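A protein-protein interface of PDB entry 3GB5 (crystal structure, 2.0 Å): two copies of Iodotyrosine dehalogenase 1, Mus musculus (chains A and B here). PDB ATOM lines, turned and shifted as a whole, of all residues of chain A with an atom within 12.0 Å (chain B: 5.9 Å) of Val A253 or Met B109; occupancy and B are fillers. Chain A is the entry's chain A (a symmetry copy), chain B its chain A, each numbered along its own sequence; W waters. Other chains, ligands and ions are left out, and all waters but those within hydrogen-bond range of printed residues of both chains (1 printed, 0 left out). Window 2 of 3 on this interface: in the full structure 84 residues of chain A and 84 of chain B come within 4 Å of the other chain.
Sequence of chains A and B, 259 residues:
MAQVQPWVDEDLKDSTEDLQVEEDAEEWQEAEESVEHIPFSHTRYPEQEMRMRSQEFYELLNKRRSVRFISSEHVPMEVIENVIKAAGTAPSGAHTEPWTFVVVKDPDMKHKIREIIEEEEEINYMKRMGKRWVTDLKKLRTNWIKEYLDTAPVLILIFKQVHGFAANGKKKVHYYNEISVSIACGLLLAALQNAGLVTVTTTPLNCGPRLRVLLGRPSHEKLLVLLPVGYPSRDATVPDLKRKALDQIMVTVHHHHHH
The backbone NH (N) of Val B103 sits at hydrogen-bond distance from the backbone carbonyl oxygen (O) of Val A251. The backbone carbonyl oxygen (O) of Val B103 lies within hydrogen-bond range of the backbone NH (N) of Val A253, 3.0 Å away.
N of Asp B108 lies close to OD2 of Asp B106. The backbone NH (N) of Met B109 sits at hydrogen-bond distance from the side-chain carboxylate (OD2) of Asp B106 (3.0 Å). A ring nitrogen (ND1) of His A254 is in hydrogen-bond range of the backbone carbonyl oxygen (O) of Thr A252 (3.1 Å).
Among the printed residues, pairs that only touch across the chains: Met A250 with Val B103, Val A251 with Val B102, Thr A252 with Val B103, Val A253 with Val B102, Val A253 with Met B109 and His A255 with Asp B106.
Of the printed residues of chain B, Met A250 touches Val B103 (3.7 Å). Of the printed residues of chain B, Val A251 touches Val B102 (3.4 Å) and Val B103 (2.8 Å). Of the printed residues of chain B, Thr A252 touches Val B103 (3.5 Å). Of the printed residues of chain B, Val A253 touches Val B102 (3.5 Å), Val B103 (3.0 Å) and Met B109 (3.7 Å). Of the printed residues of chain B, His A255 touches Asp B106 (3.3 Å). No residue of chain A comes within 4 Å of Lys B105. Of chain A, only His A255 (3.3 Å) comes within 4 Å of Asp B106. No residue of chain A comes within 4 Å of Asp B108. Printed residues of chain A within 4 Å of Met B109: Val A253 (3.7 Å). No residue of chain A comes within 4 Å of Lys B112. Ile B113 touches none of the printed residues of chain A. Leu B155 touches none of the printed residues of chain A. No residue of chain A comes within 4 Å of Leu B214. The nearest printed residue of chain B that does not touch Val A253 is Leu B215 (4.1 Å). The nearest printed residue of chain A that does not touch Met B109 is His A254 (5.5 Å). The nearest printed residue of chain B that does not touch Val A251 is Val B104 (5.6 Å).
Of the 9 printed residues of chain A, 5 touch a printed residue of chain B. Hydrophobic or aromatic side chains of chain A that line the printed part of chain B: Met A250 and Val A253. Hydrophobic or aromatic side chains of chain B within 4 Å of the printed part of chain A: Val B102, Val B103 and Met B109. Among the printed residues, no Asp or Glu carboxylate lies within 4 Å of a Lys or Arg side-chain nitrogen of the other chain.
No position is printed for both chains. Of the 8 pairs that touch across the chains among the printed residues, none has its exchanged pair printed and touching as well.
Water W1 lies within hydrogen-bond range of O of Val A253 (2.4 Å), N of Lys B105 (2.7 Å) and N of Asp B106 (2.8 Å).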
ATOM      1  N   LEU A 246     -15.141  -0.426   8.580  1.00  0.00           N
ATOM      2  CA  LEU A 246     -16.254  -0.761   9.473  1.00  0.00           C
ATOM      3  C   LEU A 246     -15.802  -0.791  10.931  1.00  0.00           C
ATOM      4  O   LEU A 246     -16.491  -0.258  11.796  1.00  0.00           O
ATOM      5  CB  LEU A 246     -16.925  -2.093   9.082  1.00  0.00           C
ATOM      6  CG  LEU A 246     -18.124  -2.535   9.956  1.00  0.00           C
ATOM      7  CD1 LEU A 246     -19.260  -1.459   9.973  1.00  0.00           C
ATOM      8  CD2 LEU A 246     -18.669  -3.901   9.483  1.00  0.00           C
ATOM      9  N   ASP A 247     -14.607  -1.336  11.197  1.00  0.00           N
ATOM     10  CA  ASP A 247     -14.173  -1.471  12.582  1.00  0.00           C
ATOM     11  C   ASP A 247     -13.827  -0.124  13.238  1.00  0.00           C
ATOM     12  O   ASP A 247     -13.716  -0.064  14.439  1.00  0.00           O
ATOM     13  CB  ASP A 247     -13.062  -2.533  12.782  1.00  0.00           C
ATOM     14  CG  ASP A 247     -11.776  -2.199  12.044  1.00  0.00           C
ATOM     15  OD1 ASP A 247     -11.657  -1.120  11.384  1.00  0.00           O
ATOM     16  OD2 ASP A 247     -10.854  -3.060  12.108  1.00  0.00           O
ATOM     17  N   ILE A 249     -15.972   2.510  12.849  1.00  0.00           N
ATOM     18  CA  ILE A 249     -17.255   3.164  13.101  1.00  0.00           C
ATOM     19  C   ILE A 249     -18.226   2.293  13.924  1.00  0.00           C
ATOM     20  O   ILE A 249     -19.230   2.775  14.432  1.00  0.00           O
ATOM     21  CB  ILE A 249     -17.931   3.636  11.812  1.00  0.00           C
ATOM     22  CG1 ILE A 249     -18.397   2.437  10.918  1.00  0.00           C
ATOM     23  CG2 ILE A 249     -17.033   4.671  11.014  1.00  0.00           C
ATOM     24  CD1 ILE A 249     -19.313   2.887   9.782  1.00  0.00           C
ATOM     25  N   MET A 250     -17.915   1.012  14.065  1.00  0.00           N
ATOM     26  CA  MET A 250     -18.886   0.077  14.672  1.00  0.00           C
ATOM     27  C   MET A 250     -18.291  -0.535  15.908  1.00  0.00           C
ATOM     28  O   MET A 250     -17.163  -1.014  15.863  1.00  0.00           O
ATOM     29  CB  MET A 250     -19.289  -1.035  13.701  1.00  0.00           C
ATOM     30  CG  MET A 250     -20.345  -2.014  14.312  1.00  0.00           C
ATOM     31  SD  MET A 250     -20.752  -3.310  13.090  1.00  0.00           S
ATOM     32  CE  MET A 250     -21.344  -4.624  14.172  1.00  0.00           C
ATOM     33  N   VAL A 251     -19.029  -0.507  17.021  1.00  0.00           N
ATOM     34  CA  VAL A 251     -18.539  -1.118  18.264  1.00  0.00           C
ATOM     35  C   VAL A 251     -19.620  -2.089  18.721  1.00  0.00           C
ATOM     36  O   VAL A 251     -20.805  -1.758  18.723  1.00  0.00           O
ATOM     37  CB  VAL A 251     -18.240  -0.068  19.392  1.00  0.00           C
ATOM     38  CG1 VAL A 251     -17.760  -0.782  20.725  1.00  0.00           C
ATOM     39  CG2 VAL A 251     -17.186   0.928  18.931  1.00  0.00           C
ATOM     40  N   THR A 252     -19.223  -3.305  19.052  1.00  0.00           N
ATOM     41  CA  THR A 252     -20.193  -4.270  19.592  1.00  0.00           C
ATOM     42  C   THR A 252     -19.980  -4.491  21.081  1.00  0.00           C
ATOM     43  O   THR A 252     -18.883  -4.876  21.503  1.00  0.00           O
ATOM     44  CB  THR A 252     -20.109  -5.638  18.887  1.00  0.00           C
ATOM     45  OG1 THR A 252     -20.278  -5.440  17.494  1.00  0.00           O
ATOM     46  CG2 THR A 252     -21.206  -6.610  19.440  1.00  0.00           C
ATOM     47  N   VAL A 253     -21.039  -4.213  21.851  1.00  0.00           N
ATOM     48  CA  VAL A 253     -21.061  -4.382  23.293  1.00  0.00           C
ATOM     49  C   VAL A 253     -21.263  -5.878  23.550  1.00  0.00           C
ATOM     50  O   VAL A 253     -22.141  -6.507  22.950  1.00  0.00           O
ATOM     51  CB  VAL A 253     -22.155  -3.501  23.917  1.00  0.00           C
ATOM     52  CG1 VAL A 253     -22.221  -3.602  25.448  1.00  0.00           C
ATOM     53  CG2 VAL A 253     -21.914  -2.078  23.523  1.00  0.00           C
ATOM     54  N   HIS A 254     -20.397  -6.465  24.360  1.00  0.00           N
ATOM     55  CA  HIS A 254     -20.488  -7.883  24.673  1.00  0.00           C
ATOM     56  C   HIS A 254     -20.904  -8.086  26.150  1.00  0.00           C
ATOM     57  O   HIS A 254     -20.912  -7.126  26.926  1.00  0.00           O
ATOM     58  CB  HIS A 254     -19.158  -8.585  24.363  1.00  0.00           C
ATOM     59  CG  HIS A 254     -18.791  -8.573  22.912  1.00  0.00           C
ATOM     60  ND1 HIS A 254     -17.924  -7.644  22.367  1.00  0.00           N
ATOM     61  CD2 HIS A 254     -19.184  -9.365  21.884  1.00  0.00           C
ATOM     62  CE1 HIS A 254     -17.796  -7.868  21.069  1.00  0.00           C
ATOM     63  NE2 HIS A 254     -18.542  -8.914  20.753  1.00  0.00           N
ATOM     64  N   HIS A 255     -21.323  -9.314  26.487  1.00  0.00           N
ATOM     65  CA  HIS A 255     -21.298  -9.890  27.876  1.00  0.00           C
ATOM     66  C   HIS A 255     -22.672 -10.332  28.417  1.00  0.00           C
ATOM     67  O   HIS A 255     -22.785 -10.875  29.555  1.00  0.00           O
ATOM     68  CB  HIS A 255     -20.566  -8.990  28.908  1.00  0.00           C
ATOM     69  CG  HIS A 255     -19.603  -9.726  29.793  1.00  0.00           C
ATOM     70  ND1 HIS A 255     -19.944 -10.215  31.042  1.00  0.00           N
ATOM     71  CD2 HIS A 255     -18.300 -10.056  29.609  1.00  0.00           C
ATOM     72  CE1 HIS A 255     -18.899 -10.820  31.580  1.00  0.00           C
ATOM     73  NE2 HIS A 255     -17.889 -10.738  30.730  1.00  0.00           N
ATOM     74  N   VAL B 102     -23.127   1.773  17.858  1.00  0.00           N
ATOM     75  CA  VAL B 102     -22.932   0.840  18.953  1.00  0.00           C
ATOM     76  C   VAL B 102     -23.999  -0.241  18.834  1.00  0.00           C
ATOM     77  O   VAL B 102     -25.192   0.030  18.898  1.00  0.00           O
ATOM     78  CB  VAL B 102     -22.964   1.566  20.330  1.00  0.00           C
ATOM     79  CG1 VAL B 102     -22.890   0.552  21.508  1.00  0.00           C
ATOM     80  CG2 VAL B 102     -21.824   2.604  20.424  1.00  0.00           C
ATOM     81  N   VAL B 103     -23.555  -1.478  18.685  1.00  0.00           N
ATOM     82  CA  VAL B 103     -24.455  -2.586  18.444  1.00  0.00           C
ATOM     83  C   VAL B 103     -24.598  -3.411  19.734  1.00  0.00           C
ATOM     84  O   VAL B 103     -23.594  -3.829  20.324  1.00  0.00           O
ATOM     85  CB  VAL B 103     -23.923  -3.446  17.249  1.00  0.00           C
ATOM     86  CG1 VAL B 103     -24.705  -4.773  17.082  1.00  0.00           C
ATOM     87  CG2 VAL B 103     -23.901  -2.586  15.943  1.00  0.00           C
ATOM     88  N   VAL B 104     -25.852  -3.602  20.173  1.00  0.00           N
ATOM     89  CA  VAL B 104     -26.142  -4.359  21.398  1.00  0.00           C
ATOM     90  C   VAL B 104     -27.067  -5.521  21.055  1.00  0.00           C
ATOM     91  O   VAL B 104     -28.194  -5.314  20.556  1.00  0.00           O
ATOM     92  CB  VAL B 104     -26.814  -3.470  22.460  1.00  0.00           C
ATOM     93  CG1 VAL B 104     -26.999  -4.228  23.816  1.00  0.00           C
ATOM     94  CG2 VAL B 104     -26.040  -2.124  22.619  1.00  0.00           C
ATOM     95  N   LYS B 105     -26.580  -6.722  21.309  1.00  0.00           N
ATOM     96  CA  LYS B 105     -27.378  -7.930  21.160  1.00  0.00           C
ATOM     97  C   LYS B 105     -27.679  -8.610  22.485  1.00  0.00           C
ATOM     98  O   LYS B 105     -28.697  -9.306  22.634  1.00  0.00           O
ATOM     99  CB  LYS B 105     -26.658  -8.892  20.230  1.00  0.00           C
ATOM    100  CG  LYS B 105     -26.636  -8.331  18.793  1.00  0.00           C
ATOM    101  CD  LYS B 105     -25.769  -9.209  17.878  1.00  0.00           C
ATOM    102  CE  LYS B 105     -24.287  -8.982  18.153  1.00  0.00           C
ATOM    103  NZ  LYS B 105     -23.413 -10.020  17.507  1.00  0.00           N
ATOM    104  N   ASP B 106     -26.780  -8.416  23.441  1.00  0.00           N
ATOM    105  CA  ASP B 106     -26.864  -9.085  24.736  1.00  0.00           C
ATOM    106  C   ASP B 106     -28.203  -8.793  25.458  1.00  0.00           C
ATOM    107  O   ASP B 106     -28.529  -7.626  25.740  1.00  0.00           O
ATOM    108  CB  ASP B 106     -25.673  -8.698  25.607  1.00  0.00           C
ATOM    109  CG  ASP B 106     -25.754  -9.305  26.981  1.00  0.00           C
ATOM    110  OD1 ASP B 106     -25.677 -10.561  27.091  1.00  0.00           O
ATOM    111  OD2 ASP B 106     -25.924  -8.537  27.948  1.00  0.00           O
ATOM    112  N   PRO B 107     -28.986  -9.857  25.759  1.00  0.00           N
ATOM    113  CA  PRO B 107     -30.284  -9.672  26.415  1.00  0.00           C
ATOM    114  C   PRO B 107     -30.227  -8.851  27.719  1.00  0.00           C
ATOM    115  O   PRO B 107     -31.080  -7.985  27.923  1.00  0.00           O
ATOM    116  CB  PRO B 107     -30.757 -11.117  26.681  1.00  0.00           C
ATOM    117  CG  PRO B 107     -30.093 -11.922  25.597  1.00  0.00           C
ATOM    118  CD  PRO B 107     -28.712 -11.283  25.479  1.00  0.00           C
ATOM    119  N   ASP B 108     -29.240  -9.095  28.582  1.00  0.00           N
ATOM    120  CA  ASP B 108     -29.140  -8.332  29.841  1.00  0.00           C
ATOM    121  C   ASP B 108     -28.909  -6.843  29.596  1.00  0.00           C
ATOM    122  O   ASP B 108     -29.553  -6.004  30.234  1.00  0.00           O
ATOM    123  CB  ASP B 108     -28.051  -8.893  30.774  1.00  0.00           C
ATOM    124  CG  ASP B 108     -28.507 -10.139  31.533  1.00  0.00           C
ATOM    125  OD1 ASP B 108     -29.743 -10.367  31.616  1.00  0.00           O
ATOM    126  OD2 ASP B 108     -27.629 -10.887  32.059  1.00  0.00           O
ATOM    127  N   MET B 109     -28.006  -6.520  28.669  1.00  0.00           N
ATOM    128  CA  MET B 109     -27.710  -5.124  28.335  1.00  0.00           C
ATOM    129  C   MET B 109     -28.910  -4.413  27.687  1.00  0.00           C
ATOM    130  O   MET B 109     -29.207  -3.276  28.036  1.00  0.00           O
ATOM    131  CB  MET B 109     -26.449  -5.020  27.457  1.00  0.00           C
ATOM    132  CG  MET B 109     -26.027  -3.577  27.096  1.00  0.00           C
ATOM    133  SD  MET B 109     -25.636  -2.542  28.526  1.00  0.00           S
ATOM    134  CE  MET B 109     -23.890  -2.905  28.722  1.00  0.00           C
ATOM    135  N   LYS B 110     -29.596  -5.083  26.761  1.00  0.00           N
ATOM    136  CA  LYS B 110     -30.810  -4.527  26.144  1.00  0.00           C
ATOM    137  C   LYS B 110     -31.886  -4.231  27.206  1.00  0.00           C
ATOM    138  O   LYS B 110     -32.578  -3.216  27.138  1.00  0.00           O
ATOM    139  CB  LYS B 110     -31.397  -5.468  25.090  1.00  0.00           C
ATOM    140  CG  LYS B 110     -30.491  -5.700  23.848  1.00  0.00           C
ATOM    141  CD  LYS B 110     -31.272  -6.328  22.702  1.00  0.00           C
ATOM    142  CE  LYS B 110     -31.529  -7.773  23.025  1.00  0.00           C
ATOM    143  NZ  LYS B 110     -32.946  -8.094  22.839  1.00  0.00           N
ATOM    144  N   HIS B 111     -32.014  -5.118  28.192  1.00  0.00           N
ATOM    145  CA  HIS B 111     -32.916  -4.856  29.307  1.00  0.00           C
ATOM    146  C   HIS B 111     -32.541  -3.627  30.172  1.00  0.00           C
ATOM    147  O   HIS B 111     -33.430  -2.849  30.558  1.00  0.00           O
ATOM    148  CB  HIS B 111     -33.164  -6.100  30.157  1.00  0.00           C
ATOM    149  CG  HIS B 111     -34.398  -5.980  30.990  1.00  0.00           C
ATOM    150  ND1 HIS B 111     -34.376  -5.999  32.365  1.00  0.00           N
ATOM    151  CD2 HIS B 111     -35.688  -5.761  30.637  1.00  0.00           C
ATOM    152  CE1 HIS B 111     -35.605  -5.827  32.826  1.00  0.00           C
ATOM    153  NE2 HIS B 111     -36.421  -5.683  31.797  1.00  0.00           N
ATOM    154  N   LYS B 112     -31.244  -3.436  30.452  1.00  0.00           N
ATOM    155  CA  LYS B 112     -30.797  -2.244  31.212  1.00  0.00           C
ATOM    156  C   LYS B 112     -31.063  -0.942  30.439  1.00  0.00           C
ATOM    157  O   LYS B 112     -31.383   0.109  31.026  1.00  0.00           O
ATOM    158  CB  LYS B 112     -29.321  -2.360  31.616  1.00  0.00           C
ATOM    159  CG  LYS B 112     -28.993  -3.392  32.731  1.00  0.00           C
ATOM    160  CD  LYS B 112     -27.528  -3.873  32.532  1.00  0.00           C
ATOM    161  CE  LYS B 112     -26.793  -4.195  33.827  1.00  0.00           C
ATOM    162  NZ  LYS B 112     -27.524  -5.132  34.743  1.00  0.00           N
ATOM    163  N   ILE B 113     -30.944  -1.016  29.117  1.00  0.00           N
ATOM    164  CA  ILE B 113     -31.255   0.113  28.244  1.00  0.00           C
ATOM    165  C   ILE B 113     -32.739   0.439  28.398  1.00  0.00           C
ATOM    166  O   ILE B 113     -33.088   1.603  28.640  1.00  0.00           O
ATOM    167  CB  ILE B 113     -30.889  -0.178  26.766  1.00  0.00           C
ATOM    168  CG1 ILE B 113     -29.338  -0.167  26.591  1.00  0.00           C
ATOM    169  CG2 ILE B 113     -31.565   0.840  25.818  1.00  0.00           C
ATOM    170  CD1 ILE B 113     -28.850  -0.792  25.243  1.00  0.00           C
ATOM    171  N   ARG B 114     -33.590  -0.593  28.281  1.00  0.00           N
ATOM    172  CA  ARG B 114     -35.037  -0.443  28.464  1.00  0.00           C
ATOM    173  C   ARG B 114     -35.392   0.149  29.833  1.00  0.00           C
ATOM    174  O   ARG B 114     -36.206   1.075  29.922  1.00  0.00           O
ATOM    175  CB  ARG B 114     -35.764  -1.777  28.252  1.00  0.00           C
ATOM    176  CG  ARG B 114     -37.284  -1.625  28.192  1.00  0.00           C
ATOM    177  CD  ARG B 114     -37.968  -2.947  28.334  1.00  0.00           C
ATOM    178  NE  ARG B 114     -39.410  -2.781  28.506  1.00  0.00           N
ATOM    179  CZ  ARG B 114     -40.282  -3.787  28.562  1.00  0.00           C
ATOM    180  NH1 ARG B 114     -39.869  -5.028  28.427  1.00  0.00           N
ATOM    181  NH2 ARG B 114     -41.574  -3.544  28.730  1.00  0.00           N
ATOM    182  N   LEU B 155     -30.014  -3.957  18.959  1.00  0.00           N
ATOM    183  CA  LEU B 155     -30.200  -2.501  19.048  1.00  0.00           C
ATOM    184  C   LEU B 155     -28.985  -1.802  18.446  1.00  0.00           C
ATOM    185  O   LEU B 155     -27.840  -2.170  18.748  1.00  0.00           O
ATOM    186  CB  LEU B 155     -30.423  -1.999  20.507  1.00  0.00           C
ATOM    187  CG  LEU B 155     -31.386  -2.747  21.428  1.00  0.00           C
ATOM    188  CD1 LEU B 155     -31.376  -2.137  22.841  1.00  0.00           C
ATOM    189  CD2 LEU B 155     -32.817  -2.792  20.836  1.00  0.00           C
ATOM    190  N   LEU B 214     -23.662   3.564  30.848  1.00  0.00           N
ATOM    191  CA  LEU B 214     -24.004   2.142  30.860  1.00  0.00           C
ATOM    192  C   LEU B 214     -23.208   1.394  29.760  1.00  0.00           C
ATOM    193  O   LEU B 214     -22.719   0.273  29.970  1.00  0.00           O
ATOM    194  CB  LEU B 214     -25.510   1.936  30.631  1.00  0.00           C
ATOM    195  CG  LEU B 214     -25.901   0.473  30.405  1.00  0.00           C
ATOM    196  CD1 LEU B 214     -25.739  -0.294  31.732  1.00  0.00           C
ATOM    197  CD2 LEU B 214     -27.308   0.329  29.812  1.00  0.00           C
ATOM    198  N   LEU B 215     -23.075   2.026  28.601  1.00  0.00           N
ATOM    199  CA  LEU B 215     -22.387   1.379  27.477  1.00  0.00           C
ATOM    200  C   LEU B 215     -20.857   1.627  27.441  1.00  0.00           C
ATOM    201  O   LEU B 215     -20.182   1.144  26.540  1.00  0.00           O
ATOM    202  CB  LEU B 215     -23.082   1.727  26.139  1.00  0.00           C
ATOM    203  CG  LEU B 215     -24.554   1.256  26.081  1.00  0.00           C
ATOM    204  CD1 LEU B 215     -25.287   1.863  24.937  1.00  0.00           C
ATOM    205  CD2 LEU B 215     -24.668  -0.282  25.977  1.00  0.00           C
HETATM  206  O   HOH W   1     -24.285  -7.589  22.500  1.00  0.00           O
